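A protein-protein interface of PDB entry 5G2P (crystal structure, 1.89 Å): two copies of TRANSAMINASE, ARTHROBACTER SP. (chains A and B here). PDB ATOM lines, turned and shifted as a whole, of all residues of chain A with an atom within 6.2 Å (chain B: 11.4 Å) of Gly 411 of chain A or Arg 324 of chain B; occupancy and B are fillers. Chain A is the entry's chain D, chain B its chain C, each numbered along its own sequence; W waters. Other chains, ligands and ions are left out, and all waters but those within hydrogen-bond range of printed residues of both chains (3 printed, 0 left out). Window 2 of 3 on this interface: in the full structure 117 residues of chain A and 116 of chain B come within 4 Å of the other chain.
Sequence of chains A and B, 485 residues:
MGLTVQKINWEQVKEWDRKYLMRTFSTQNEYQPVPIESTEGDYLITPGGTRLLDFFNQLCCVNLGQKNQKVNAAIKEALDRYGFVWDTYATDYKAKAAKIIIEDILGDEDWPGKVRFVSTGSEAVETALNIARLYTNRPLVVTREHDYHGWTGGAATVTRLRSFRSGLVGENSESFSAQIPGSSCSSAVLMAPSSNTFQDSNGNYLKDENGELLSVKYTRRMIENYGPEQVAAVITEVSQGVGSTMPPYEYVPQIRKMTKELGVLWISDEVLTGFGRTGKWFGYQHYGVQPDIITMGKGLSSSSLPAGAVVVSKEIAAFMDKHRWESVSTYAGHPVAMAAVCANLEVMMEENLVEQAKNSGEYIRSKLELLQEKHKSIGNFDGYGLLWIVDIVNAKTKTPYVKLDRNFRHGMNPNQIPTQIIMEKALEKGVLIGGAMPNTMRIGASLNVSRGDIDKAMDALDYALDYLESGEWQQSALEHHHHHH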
ATOM      1  N   THR A  24     -34.517  15.177 -23.753  1.00  0.00           N
ATOM      2  CA  THR A  24     -33.355  14.733 -24.541  1.00  0.00           C
ATOM      3  C   THR A  24     -32.355  15.870 -24.703  1.00  0.00           C
ATOM      4  O   THR A  24     -32.763  17.026 -24.859  1.00  0.00           O
ATOM      5  CB  THR A  24     -33.756  14.194 -25.928  1.00  0.00           C
ATOM      6  OG1 THR A  24     -34.579  15.153 -26.573  1.00  0.00           O
ATOM      7  CG2 THR A  24     -34.527  12.857 -25.813  1.00  0.00           C
ATOM      8  N   PHE A  25     -31.060  15.534 -24.662  1.00  0.00           N
ATOM      9  CA  PHE A  25     -29.924  16.488 -24.799  1.00  0.00           C
ATOM     10  C   PHE A  25     -29.748  17.501 -23.649  1.00  0.00           C
ATOM     11  O   PHE A  25     -28.665  18.058 -23.485  1.00  0.00           O
ATOM     12  CB  PHE A  25     -29.907  17.170 -26.169  1.00  0.00           C
ATOM     13  CG  PHE A  25     -29.837  16.199 -27.313  1.00  0.00           C
ATOM     14  CD1 PHE A  25     -28.609  15.674 -27.725  1.00  0.00           C
ATOM     15  CD2 PHE A  25     -30.992  15.796 -27.968  1.00  0.00           C
ATOM     16  CE1 PHE A  25     -28.539  14.760 -28.777  1.00  0.00           C
ATOM     17  CE2 PHE A  25     -30.927  14.892 -29.014  1.00  0.00           C
ATOM     18  CZ  PHE A  25     -29.699  14.361 -29.410  1.00  0.00           C
ATOM     19  N   SER A  26     -30.797  17.673 -22.838  1.00  0.00           N
ATOM     20  CA  SER A  26     -30.819  18.623 -21.730  1.00  0.00           C
ATOM     21  C   SER A  26     -31.205  17.916 -20.469  1.00  0.00           C
ATOM     22  O   SER A  26     -32.133  17.110 -20.479  1.00  0.00           O
ATOM     23  CB  SER A  26     -31.877  19.692 -21.968  1.00  0.00           C
ATOM     24  OG  SER A  26     -31.409  20.606 -22.910  1.00  0.00           O
ATOM     25  N   THR A  27     -30.512  18.206 -19.367  1.00  0.00           N
ATOM     26  CA  THR A  27     -31.017  17.734 -18.084  1.00  0.00           C
ATOM     27  C   THR A  27     -32.290  18.524 -17.756  1.00  0.00           C
ATOM     28  O   THR A  27     -32.511  19.613 -18.305  1.00  0.00           O
ATOM     29  CB  THR A  27     -30.017  17.924 -16.930  1.00  0.00           C
ATOM     30  OG1 THR A  27     -29.810  19.322 -16.734  1.00  0.00           O
ATOM     31  CG2 THR A  27     -28.688  17.227 -17.215  1.00  0.00           C
ATOM     32  N   GLU A  30     -31.381  22.056 -16.337  1.00  0.00           N
ATOM     33  CA  GLU A  30     -30.968  23.156 -17.210  1.00  0.00           C
ATOM     34  C   GLU A  30     -32.000  23.499 -18.291  1.00  0.00           C
ATOM     35  O   GLU A  30     -31.812  24.465 -19.045  1.00  0.00           O
ATOM     36  CB  GLU A  30     -29.621  22.825 -17.880  1.00  0.00           C
ATOM     37  CG  GLU A  30     -29.735  21.751 -18.966  1.00  0.00           C
ATOM     38  CD  GLU A  30     -28.399  21.192 -19.397  1.00  0.00           C
ATOM     39  OE1 GLU A  30     -27.417  21.938 -19.433  1.00  0.00           O
ATOM     40  OE2 GLU A  30     -28.324  19.990 -19.707  1.00  0.00           O
ATOM     41  N   GLY A 167     -27.043   7.073 -25.590  1.00  0.00           N
ATOM     42  CA  GLY A 167     -26.462   6.936 -24.265  1.00  0.00           C
ATOM     43  C   GLY A 167     -26.722   8.172 -23.398  1.00  0.00           C
ATOM     44  O   GLY A 167     -27.417   9.116 -23.823  1.00  0.00           O
ATOM     45  N   LEU A 168     -26.146   8.169 -22.202  1.00  0.00           N
ATOM     46  CA  LEU A 168     -26.306   9.287 -21.262  1.00  0.00           C
ATOM     47  C   LEU A 168     -25.000  10.007 -20.944  1.00  0.00           C
ATOM     48  O   LEU A 168     -23.936   9.386 -20.846  1.00  0.00           O
ATOM     49  CB  LEU A 168     -26.914   8.787 -19.961  1.00  0.00           C
ATOM     50  CG  LEU A 168     -28.270   8.084 -20.018  1.00  0.00           C
ATOM     51  CD1 LEU A 168     -28.524   7.466 -18.653  1.00  0.00           C
ATOM     52  CD2 LEU A 168     -29.369   9.060 -20.397  1.00  0.00           C
ATOM     53  N   VAL A 169     -25.072  11.320 -20.767  1.00  0.00           N
ATOM     54  CA  VAL A 169     -23.921  12.045 -20.228  1.00  0.00           C
ATOM     55  C   VAL A 169     -24.392  12.988 -19.119  1.00  0.00           C
ATOM     56  O   VAL A 169     -25.601  13.274 -18.973  1.00  0.00           O
ATOM     57  CB  VAL A 169     -23.107  12.797 -21.315  1.00  0.00           C
ATOM     58  CG1 VAL A 169     -22.402  11.831 -22.269  1.00  0.00           C
ATOM     59  CG2 VAL A 169     -23.987  13.744 -22.094  1.00  0.00           C
ATOM     60  N   GLY A 170     -23.439  13.472 -18.328  1.00  0.00           N
ATOM     61  CA  GLY A 170     -23.775  14.379 -17.254  1.00  0.00           C
ATOM     62  C   GLY A 170     -23.926  15.816 -17.713  1.00  0.00           C
ATOM     63  O   GLY A 170     -23.703  16.130 -18.897  1.00  0.00           O
ATOM     64  N   GLU A 171     -24.287  16.685 -16.763  1.00  0.00           N
ATOM     65  CA  GLU A 171     -24.421  18.125 -17.000  1.00  0.00           C
ATOM     66  C   GLU A 171     -23.096  18.847 -16.792  1.00  0.00           C
ATOM     67  O   GLU A 171     -22.677  19.070 -15.650  1.00  0.00           O
ATOM     68  CB  GLU A 171     -25.454  18.719 -16.067  1.00  0.00           C
ATOM     69  CG  GLU A 171     -25.949  20.096 -16.491  1.00  0.00           C
ATOM     70  CD  GLU A 171     -26.882  20.695 -15.459  1.00  0.00           C
ATOM     71  OE1 GLU A 171     -27.949  20.114 -15.182  1.00  0.00           O
ATOM     72  OE2 GLU A 171     -26.529  21.743 -14.908  1.00  0.00           O
ATOM     73  N   ASN A 172     -22.436  19.217 -17.892  1.00  0.00           N
ATOM     74  CA  ASN A 172     -21.106  19.827 -17.813  1.00  0.00           C
ATOM     75  C   ASN A 172     -20.151  18.992 -16.961  1.00  0.00           C
ATOM     76  O   ASN A 172     -19.452  19.516 -16.111  1.00  0.00           O
ATOM     77  CB  ASN A 172     -21.215  21.264 -17.293  1.00  0.00           C
ATOM     78  CG  ASN A 172     -22.303  22.047 -18.002  1.00  0.00           C
ATOM     79  OD1 ASN A 172     -22.416  21.997 -19.228  1.00  0.00           O
ATOM     80  ND2 ASN A 172     -23.132  22.745 -17.234  1.00  0.00           N
ATOM     81  N   SER A 173     -20.125  17.684 -17.208  1.00  0.00           N
ATOM     82  CA  SER A 173     -19.314  16.761 -16.434  1.00  0.00           C
ATOM     83  C   SER A 173     -18.955  15.529 -17.271  1.00  0.00           C
ATOM     84  O   SER A 173     -19.709  15.144 -18.166  1.00  0.00           O
ATOM     85  CB  SER A 173     -20.066  16.320 -15.164  1.00  0.00           C
ATOM     86  OG  SER A 173     -19.403  15.225 -14.547  1.00  0.00           O
ATOM     87  N   GLU A 174     -17.803  14.929 -16.962  1.00  0.00           N
ATOM     88  CA  GLU A 174     -17.367  13.659 -17.548  1.00  0.00           C
ATOM     89  C   GLU A 174     -17.659  12.457 -16.657  1.00  0.00           C
ATOM     90  O   GLU A 174     -17.263  11.338 -16.981  1.00  0.00           O
ATOM     91  CB  GLU A 174     -15.856  13.715 -17.861  1.00  0.00           C
ATOM     92  CG  GLU A 174     -15.498  14.703 -18.973  1.00  0.00           C
ATOM     93  CD  GLU A 174     -16.329  14.481 -20.230  1.00  0.00           C
ATOM     94  OE1 GLU A 174     -16.395  13.308 -20.676  1.00  0.00           O
ATOM     95  OE2 GLU A 174     -16.934  15.457 -20.755  1.00  0.00           O
ATOM     96  N   SER A 177     -21.168   9.445 -17.669  1.00  0.00           N
ATOM     97  CA  SER A 177     -21.243   8.991 -19.046  1.00  0.00           C
ATOM     98  C   SER A 177     -21.481   7.477 -19.130  1.00  0.00           C
ATOM     99  O   SER A 177     -20.822   6.678 -18.450  1.00  0.00           O
ATOM    100  CB  SER A 177     -19.989   9.410 -19.812  1.00  0.00           C
ATOM    101  OG  SER A 177     -19.948  10.831 -19.870  1.00  0.00           O
ATOM    102  N   ARG A 409     -18.664  13.977 -26.949  1.00  0.00           N
ATOM    103  CA  ARG A 409     -20.004  13.697 -26.443  1.00  0.00           C
ATOM    104  C   ARG A 409     -20.577  14.955 -25.775  1.00  0.00           C
ATOM    105  O   ARG A 409     -19.852  15.936 -25.585  1.00  0.00           O
ATOM    106  CB  ARG A 409     -20.020  12.499 -25.510  1.00  0.00           C
ATOM    107  CG  ARG A 409     -19.812  11.169 -26.247  1.00  0.00           C
ATOM    108  CD  ARG A 409     -19.934  10.021 -25.261  1.00  0.00           C
ATOM    109  NE  ARG A 409     -21.323   9.676 -24.986  1.00  0.00           N
ATOM    110  CZ  ARG A 409     -21.707   8.813 -24.056  1.00  0.00           C
ATOM    111  NH1 ARG A 409     -20.800   8.219 -23.286  1.00  0.00           N
ATOM    112  NH2 ARG A 409     -22.997   8.543 -23.910  1.00  0.00           N
ATOM    113  N   HIS A 410     -21.868  14.915 -25.420  1.00  0.00           N
ATOM    114  CA  HIS A 410     -22.577  16.103 -24.924  1.00  0.00           C
ATOM    115  C   HIS A 410     -22.364  16.429 -23.422  1.00  0.00           C
ATOM    116  O   HIS A 410     -23.075  17.269 -22.883  1.00  0.00           O
ATOM    117  CB  HIS A 410     -24.082  16.047 -25.249  1.00  0.00           C
ATOM    118  CG  HIS A 410     -24.396  16.025 -26.719  1.00  0.00           C
ATOM    119  ND1 HIS A 410     -24.464  14.856 -27.449  1.00  0.00           N
ATOM    120  CD2 HIS A 410     -24.690  17.026 -27.584  1.00  0.00           C
ATOM    121  CE1 HIS A 410     -24.789  15.135 -28.698  1.00  0.00           C
ATOM    122  NE2 HIS A 410     -24.920  16.446 -28.814  1.00  0.00           N
ATOM    123  N   GLY A 411     -21.396  15.783 -22.766  1.00  0.00           N
ATOM    124  CA  GLY A 411     -21.031  16.102 -21.368  1.00  0.00           C
ATOM    125  C   GLY A 411     -20.383  17.485 -21.239  1.00  0.00           C
ATOM    126  O   GLY A 411     -20.424  18.099 -20.172  1.00  0.00           O
ATOM    127  N   MET A 412     -19.789  17.956 -22.336  1.00  0.00           N
ATOM    128  CA  MET A 412     -19.153  19.270 -22.417  1.00  0.00           C
ATOM    129  C   MET A 412     -20.089  20.425 -22.105  1.00  0.00           C
ATOM    130  O   MET A 412     -21.288  20.363 -22.389  1.00  0.00           O
ATOM    131  CB  MET A 412     -18.644  19.527 -23.838  1.00  0.00           C
ATOM    132  CG  MET A 412     -17.413  18.778 -24.266  1.00  0.00           C
ATOM    133  SD  MET A 412     -16.965  19.452 -25.880  1.00  0.00           S
ATOM    134  CE  MET A 412     -16.211  21.011 -25.353  1.00  0.00           C
ATOM    135  N   ASN A 413     -19.518  21.500 -21.563  1.00  0.00           N
ATOM    136  CA  ASN A 413     -20.237  22.741 -21.356  1.00  0.00           C
ATOM    137  C   ASN A 413     -20.473  23.428 -22.702  1.00  0.00           C
ATOM    138  O   ASN A 413     -19.509  23.709 -23.408  1.00  0.00           O
ATOM    139  CB  ASN A 413     -19.406  23.648 -20.444  1.00  0.00           C
ATOM    140  CG  ASN A 413     -20.226  24.730 -19.787  1.00  0.00           C
ATOM    141  OD1 ASN A 413     -21.082  25.352 -20.412  1.00  0.00           O
ATOM    142  ND2 ASN A 413     -19.967  24.959 -18.512  1.00  0.00           N
ATOM    143  N   PRO A 414     -21.753  23.678 -23.069  1.00  0.00           N
ATOM    144  CA  PRO A 414     -22.109  24.388 -24.307  1.00  0.00           C
ATOM    145  C   PRO A 414     -21.429  25.759 -24.473  1.00  0.00           C
ATOM    146  O   PRO A 414     -21.246  26.207 -25.609  1.00  0.00           O
ATOM    147  CB  PRO A 414     -23.637  24.568 -24.190  1.00  0.00           C
ATOM    148  CG  PRO A 414     -23.949  24.358 -22.743  1.00  0.00           C
ATOM    149  CD  PRO A 414     -22.963  23.312 -22.310  1.00  0.00           C
ATOM    150  N   LYS B 114     -43.250  10.158 -16.500  1.00  0.00           N
ATOM    151  CA  LYS B 114     -43.067  10.928 -17.708  1.00  0.00           C
ATOM    152  C   LYS B 114     -43.337  10.079 -18.957  1.00  0.00           C
ATOM    153  O   LYS B 114     -43.358   8.836 -18.905  1.00  0.00           O
ATOM    154  CB  LYS B 114     -41.633  11.480 -17.746  1.00  0.00           C
ATOM    155  CG  LYS B 114     -41.419  12.771 -16.961  1.00  0.00           C
ATOM    156  CD  LYS B 114     -40.008  13.311 -17.149  1.00  0.00           C
ATOM    157  CE  LYS B 114     -39.964  14.783 -16.776  1.00  0.00           C
ATOM    158  NZ  LYS B 114     -38.803  15.480 -17.415  1.00  0.00           N
ATOM    159  N   ARG B 116     -42.360   9.587 -23.276  1.00  0.00           N
ATOM    160  CA  ARG B 116     -41.673   9.967 -24.522  1.00  0.00           C
ATOM    161  C   ARG B 116     -42.505   9.497 -25.701  1.00  0.00           C
ATOM    162  O   ARG B 116     -42.852   8.307 -25.797  1.00  0.00           O
ATOM    163  CB  ARG B 116     -40.248   9.374 -24.609  1.00  0.00           C
ATOM    164  CG  ARG B 116     -39.596   9.553 -25.978  1.00  0.00           C
ATOM    165  CD  ARG B 116     -38.073   9.527 -25.905  1.00  0.00           C
ATOM    166  NE  ARG B 116     -37.450   9.604 -27.238  1.00  0.00           N
ATOM    167  CZ  ARG B 116     -37.317  10.734 -27.938  1.00  0.00           C
ATOM    168  NH1 ARG B 116     -37.775  11.882 -27.444  1.00  0.00           N
ATOM    169  NH2 ARG B 116     -36.710  10.734 -29.131  1.00  0.00           N
ATOM    170  N   ILE B 131     -34.103   2.521 -22.204  1.00  0.00           N
ATOM    171  CA  ILE B 131     -34.305   3.075 -20.862  1.00  0.00           C
ATOM    172  C   ILE B 131     -34.045   2.040 -19.755  1.00  0.00           C
ATOM    173  O   ILE B 131     -33.339   2.339 -18.786  1.00  0.00           O
ATOM    174  CB  ILE B 131     -35.708   3.702 -20.721  1.00  0.00           C
ATOM    175  CG1 ILE B 131     -35.833   4.888 -21.681  1.00  0.00           C
ATOM    176  CG2 ILE B 131     -36.010   4.141 -19.271  1.00  0.00           C
ATOM    177  CD1 ILE B 131     -37.243   5.402 -21.806  1.00  0.00           C
ATOM    178  N   LEU B 134     -30.271   1.348 -19.487  1.00  0.00           N
ATOM    179  CA  LEU B 134     -29.574   2.507 -18.939  1.00  0.00           C
ATOM    180  C   LEU B 134     -29.865   2.722 -17.456  1.00  0.00           C
ATOM    181  O   LEU B 134     -28.944   2.980 -16.665  1.00  0.00           O
ATOM    182  CB  LEU B 134     -29.896   3.784 -19.723  1.00  0.00           C
ATOM    183  CG  LEU B 134     -29.274   3.953 -21.111  1.00  0.00           C
ATOM    184  CD1 LEU B 134     -29.998   5.067 -21.869  1.00  0.00           C
ATOM    185  CD2 LEU B 134     -27.767   4.209 -21.036  1.00  0.00           C
ATOM    186  N   ILE B 316     -37.658   6.044 -12.454  1.00  0.00           N
ATOM    187  CA  ILE B 316     -36.952   6.048 -13.744  1.00  0.00           C
ATOM    188  C   ILE B 316     -36.857   7.443 -14.341  1.00  0.00           C
ATOM    189  O   ILE B 316     -35.786   7.850 -14.754  1.00  0.00           O
ATOM    190  CB  ILE B 316     -37.567   5.037 -14.720  1.00  0.00           C
ATOM    191  CG1 ILE B 316     -37.384   3.616 -14.157  1.00  0.00           C
ATOM    192  CG2 ILE B 316     -36.971   5.195 -16.133  1.00  0.00           C
ATOM    193  CD1 ILE B 316     -38.149   2.551 -14.935  1.00  0.00           C
ATOM    194  N   ALA B 317     -37.966   8.190 -14.381  1.00  0.00           N
ATOM    195  CA  ALA B 317     -37.911   9.596 -14.866  1.00  0.00           C
ATOM    196  C   ALA B 317     -36.907  10.475 -14.122  1.00  0.00           C
ATOM    197  O   ALA B 317     -36.213  11.292 -14.744  1.00  0.00           O
ATOM    198  CB  ALA B 317     -39.298  10.243 -14.848  1.00  0.00           C
ATOM    199  N   ALA B 318     -36.850  10.333 -12.790  1.00  0.00           N
ATOM    200  CA  ALA B 318     -35.921  11.126 -11.965  1.00  0.00           C
ATOM    201  C   ALA B 318     -34.461  10.823 -12.337  1.00  0.00           C
ATOM    202  O   ALA B 318     -33.665  11.745 -12.465  1.00  0.00           O
ATOM    203  CB  ALA B 318     -36.155  10.890 -10.481  1.00  0.00           C
ATOM    204  N   PHE B 319     -34.125   9.548 -12.548  1.00  0.00           N
ATOM    205  CA  PHE B 319     -32.801   9.172 -13.048  1.00  0.00           C
ATOM    206  C   PHE B 319     -32.505   9.792 -14.424  1.00  0.00           C
ATOM    207  O   PHE B 319     -31.486  10.462 -14.600  1.00  0.00           O
ATOM    208  CB  PHE B 319     -32.665   7.641 -13.088  1.00  0.00           C
ATOM    209  CG  PHE B 319     -31.412   7.150 -13.760  1.00  0.00           C
ATOM    210  CD1 PHE B 319     -30.246   6.966 -13.025  1.00  0.00           C
ATOM    211  CD2 PHE B 319     -31.401   6.862 -15.130  1.00  0.00           C
ATOM    212  CE1 PHE B 319     -29.086   6.499 -13.635  1.00  0.00           C
ATOM    213  CE2 PHE B 319     -30.243   6.395 -15.745  1.00  0.00           C
ATOM    214  CZ  PHE B 319     -29.082   6.217 -15.005  1.00  0.00           C
ATOM    215  N   MET B 320     -33.406   9.614 -15.393  1.00  0.00           N
ATOM    216  CA  MET B 320     -33.163  10.105 -16.753  1.00  0.00           C
ATOM    217  C   MET B 320     -33.029  11.647 -16.787  1.00  0.00           C
ATOM    218  O   MET B 320     -32.160  12.179 -17.496  1.00  0.00           O
ATOM    219  CB  MET B 320     -34.253   9.598 -17.695  1.00  0.00           C
ATOM    220  CG  MET B 320     -34.280   8.067 -17.793  1.00  0.00           C
ATOM    221  SD  MET B 320     -32.883   7.388 -18.719  1.00  0.00           S
ATOM    222  CE  MET B 320     -33.089   8.260 -20.280  1.00  0.00           C
ATOM    223  N   ASP B 321     -33.864  12.332 -15.994  1.00  0.00           N
ATOM    224  CA  ASP B 321     -33.827  13.799 -15.777  1.00  0.00           C
ATOM    225  C   ASP B 321     -32.477  14.358 -15.307  1.00  0.00           C
ATOM    226  O   ASP B 321     -32.184  15.532 -15.520  1.00  0.00           O
ATOM    227  CB  ASP B 321     -34.879  14.214 -14.733  1.00  0.00           C
ATOM    228  CG  ASP B 321     -36.295  14.330 -15.317  1.00  0.00           C
ATOM    229  OD1 ASP B 321     -36.479  14.253 -16.558  1.00  0.00           O
ATOM    230  OD2 ASP B 321     -37.232  14.524 -14.513  1.00  0.00           O
ATOM    231  N   LYS B 322     -31.663  13.529 -14.656  1.00  0.00           N
ATOM    232  CA  LYS B 322     -30.352  13.965 -14.190  1.00  0.00           C
ATOM    233  C   LYS B 322     -29.241  13.911 -15.246  1.00  0.00           C
ATOM    234  O   LYS B 322     -28.086  14.234 -14.943  1.00  0.00           O
ATOM    235  CB  LYS B 322     -29.973  13.149 -12.949  1.00  0.00           C
ATOM    236  CG  LYS B 322     -30.696  13.659 -11.708  1.00  0.00           C
ATOM    237  CD  LYS B 322     -30.846  12.577 -10.653  1.00  0.00           C
ATOM    238  CE  LYS B 322     -32.001  12.920  -9.709  1.00  0.00           C
ATOM    239  NZ  LYS B 322     -32.380  11.806  -8.790  1.00  0.00           N
ATOM    240  N   HIS B 323     -29.585  13.514 -16.477  1.00  0.00           N
ATOM    241  CA  HIS B 323     -28.598  13.253 -17.528  1.00  0.00           C
ATOM    242  C   HIS B 323     -29.009  13.960 -18.793  1.00  0.00           C
ATOM    243  O   HIS B 323     -30.197  14.240 -18.988  1.00  0.00           O
ATOM    244  CB  HIS B 323     -28.499  11.750 -17.876  1.00  0.00           C
ATOM    245  CG  HIS B 323     -27.990  10.876 -16.767  1.00  0.00           C
ATOM    246  ND1 HIS B 323     -28.821  10.338 -15.805  1.00  0.00           N
ATOM    247  CD2 HIS B 323     -26.743  10.420 -16.488  1.00  0.00           C
ATOM    248  CE1 HIS B 323     -28.101   9.610 -14.965  1.00  0.00           C
ATOM    249  NE2 HIS B 323     -26.840   9.636 -15.363  1.00  0.00           N
ATOM    250  N   ARG B 324     -28.034  14.209 -19.668  1.00  0.00           N
ATOM    251  CA  ARG B 324     -28.328  14.586 -21.050  1.00  0.00           C
ATOM    252  C   ARG B 324     -28.426  13.285 -21.867  1.00  0.00           C
ATOM    253  O   ARG B 324     -27.443  12.539 -21.980  1.00  0.00           O
ATOM    254  CB  ARG B 324     -27.249  15.509 -21.599  1.00  0.00           C
ATOM    255  CG  ARG B 324     -27.130  16.843 -20.865  1.00  0.00           C
ATOM    256  CD  ARG B 324     -25.840  17.576 -21.211  1.00  0.00           C
ATOM    257  NE  ARG B 324     -25.871  18.946 -20.711  1.00  0.00           N
ATOM    258  CZ  ARG B 324     -24.819  19.749 -20.576  1.00  0.00           C
ATOM    259  NH1 ARG B 324     -23.585  19.335 -20.877  1.00  0.00           N
ATOM    260  NH2 ARG B 324     -25.008  20.981 -20.120  1.00  0.00           N
ATOM    261  N   TRP B 325     -29.615  13.002 -22.398  1.00  0.00           N
ATOM    262  CA  TRP B 325     -29.860  11.779 -23.197  1.00  0.00           C
ATOM    263  C   TRP B 325     -29.627  12.033 -24.700  1.00  0.00           C
ATOM    264  O   TRP B 325     -30.276  12.900 -25.310  1.00  0.00           O
ATOM    265  CB  TRP B 325     -31.274  11.310 -22.936  1.00  0.00           C
ATOM    266  CG  TRP B 325     -31.630   9.926 -23.453  1.00  0.00           C
ATOM    267  CD1 TRP B 325     -30.780   8.917 -23.833  1.00  0.00           C
ATOM    268  CD2 TRP B 325     -32.956   9.397 -23.548  1.00  0.00           C
ATOM    269  NE1 TRP B 325     -31.516   7.794 -24.206  1.00  0.00           N
ATOM    270  CE2 TRP B 325     -32.848   8.066 -24.032  1.00  0.00           C
ATOM    271  CE3 TRP B 325     -34.232   9.930 -23.280  1.00  0.00           C
ATOM    272  CZ2 TRP B 325     -33.965   7.266 -24.257  1.00  0.00           C
ATOM    273  CZ3 TRP B 325     -35.348   9.137 -23.508  1.00  0.00           C
ATOM    274  CH2 TRP B 325     -35.206   7.816 -24.000  1.00  0.00           C
ATOM    275  N   GLU B 326     -28.669  11.305 -25.271  1.00  0.00           N
ATOM    276  CA  GLU B 326     -28.185  11.569 -26.629  1.00  0.00           C
ATOM    277  C   GLU B 326     -28.989  10.811 -27.693  1.00  0.00           C
ATOM    278  O   GLU B 326     -28.429  10.046 -28.476  1.00  0.00           O
ATOM    279  CB  GLU B 326     -26.695  11.243 -26.737  1.00  0.00           C
ATOM    280  CG  GLU B 326     -25.827  12.086 -25.820  1.00  0.00           C
ATOM    281  CD  GLU B 326     -24.355  11.747 -25.908  1.00  0.00           C
ATOM    282  OE1 GLU B 326     -24.001  10.563 -25.746  1.00  0.00           O
ATOM    283  OE2 GLU B 326     -23.546  12.665 -26.144  1.00  0.00           O
ATOM    284  N   SER B 327     -30.301  11.056 -27.724  1.00  0.00           N
ATOM    285  CA  SER B 327     -31.211  10.276 -28.568  1.00  0.00           C
ATOM    286  C   SER B 327     -32.099  11.229 -29.349  1.00  0.00           C
ATOM    287  O   SER B 327     -32.806  12.065 -28.750  1.00  0.00           O
ATOM    288  CB  SER B 327     -32.070   9.327 -27.713  1.00  0.00           C
ATOM    289  OG  SER B 327     -32.655   8.293 -28.507  1.00  0.00           O
ATOM    290  N   VAL B 328     -32.003  11.142 -30.676  1.00  0.00           N
ATOM    291  CA  VAL B 328     -32.910  11.885 -31.559  1.00  0.00           C
ATOM    292  C   VAL B 328     -33.653  10.964 -32.533  1.00  0.00           C
ATOM    293  O   VAL B 328     -33.075  10.035 -33.106  1.00  0.00           O
ATOM    294  CB  VAL B 328     -32.212  13.043 -32.324  1.00  0.00           C
ATOM    295  CG1 VAL B 328     -31.055  12.538 -33.214  1.00  0.00           C
ATOM    296  CG2 VAL B 328     -33.237  13.821 -33.151  1.00  0.00           C
HETATM  297  O   HOH W   1     -31.829  14.468 -21.516  1.00  0.00           O
HETATM  298  O   HOH W   2     -24.741   8.110 -27.080  1.00  0.00           O
HETATM  299  O   HOH W   3     -34.456  14.257 -29.187  1.00  0.00           O
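N of Thr 27 of chain A touches CG of Arg 324 of chain B (3.9 Å).
Leu 168 of chain A touches Arg 324 of chain B.
CA of His 323 of chain B touches O of Val 169 of chain A (3.3 Å).
Arg 324 of chain B touches Gly 170 of chain A.
ND1 of His 410 of chain A lies within hydrogen-bond range of OE2 of Glu 326 of chain B (2.7 Å).
The guanidinium group (NH1) of Arg 324 of chain B lies within hydrogen-bond range of the backbone carbonyl oxygen (O) of Met 412 of chain A.
O of Gly 411 of chain A is in hydrogen-bond range of NH1 of Arg 324 of chain B, at 3.5 Å.
The backbone NH of Arg 324 of chain B sits at hydrogen-bond distance from the backbone carbonyl oxygen of Val 169 of chain A (2.7 Å).
NH1 of Arg 324 of chain B is in hydrogen-bond range of O of His 410 of chain A.
The side-chain carboxylate of Glu 326 of chain B lies within salt-bridge range of the guanidinium group of Arg 409 of chain A, at 2.9 Å.
O of Trp 325 of chain B sits at hydrogen-bond distance from N of Phe 25 of chain A, at 2.8 Å.
The backbone carbonyl oxygen (O) of Gly 167 of chain A lies within hydrogen-bond range of the backbone NH (N) of Glu 326 of chain B (2.9 Å).
NH2 of Arg 324 of chain B lies within salt-bridge range of OE1 of Glu 30 of chain A (2.7 Å).
The guanidinium group of Arg 324 of chain B sits at hydrogen-bond distance from the side-chain amide oxygen of Asn 172 of chain A (2.9 Å).
Of the printed residues of chain B, Thr 24 of chain A touches Arg 116, Trp 325 and Ser 327.
Thr 27 of chain A touches just these residues of chain B: Asp 321, Lys 322, His 323 and Arg 324.
Leu 168 of chain A touches just these residues of chain B: Leu 134, Phe 319, Met 320, His 323, Arg 324 and Trp 325.
Printed residues of chain A within 4 Å of Ser 327 of chain B: Thr 24 (3.5 Å) and Phe 25 (3.4 Å).
The nearest residue of chain A that does not touch Arg 324 of chain B is Ser 26 of chain A (4.2 Å).
Of the 20 printed residues of chain A, 16 touch a printed residue of chain B.
Hydrophobic or aromatic side chains of chain A within 4 Å of the printed part of chain B: Phe 25, Leu 168, Val 169, His 410 and Pro 414.
Along chain A the printed residues that touch a printed residue of chain B span positions 24 to 414.
No position is printed for both chains.
Of the 33 pairs that touch across the chains among the printed residues, none has its exchanged pair printed and touching as well.
OG1 of Thr 27 of chain A is in hydrogen-bond range of OE1 of Glu 171 of chain A (2.5 Å).
The side-chain amino group (NZ) of Lys 114 of chain B lies within salt-bridge range of the side-chain carboxylate (OD1) of Asp 321 of chain B.
Water W3 bridges the side-chain hydroxyl of Thr 24 of chain A (2.8 Å) and the backbone carbonyl oxygen of Ser 327 of chain B (2.8 Å).
Water W2 bridges the side-chain carboxylate of Glu 326 of chain B (2.9 Å) and the backbone NH of Gly 167 of chain A (2.9 Å).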
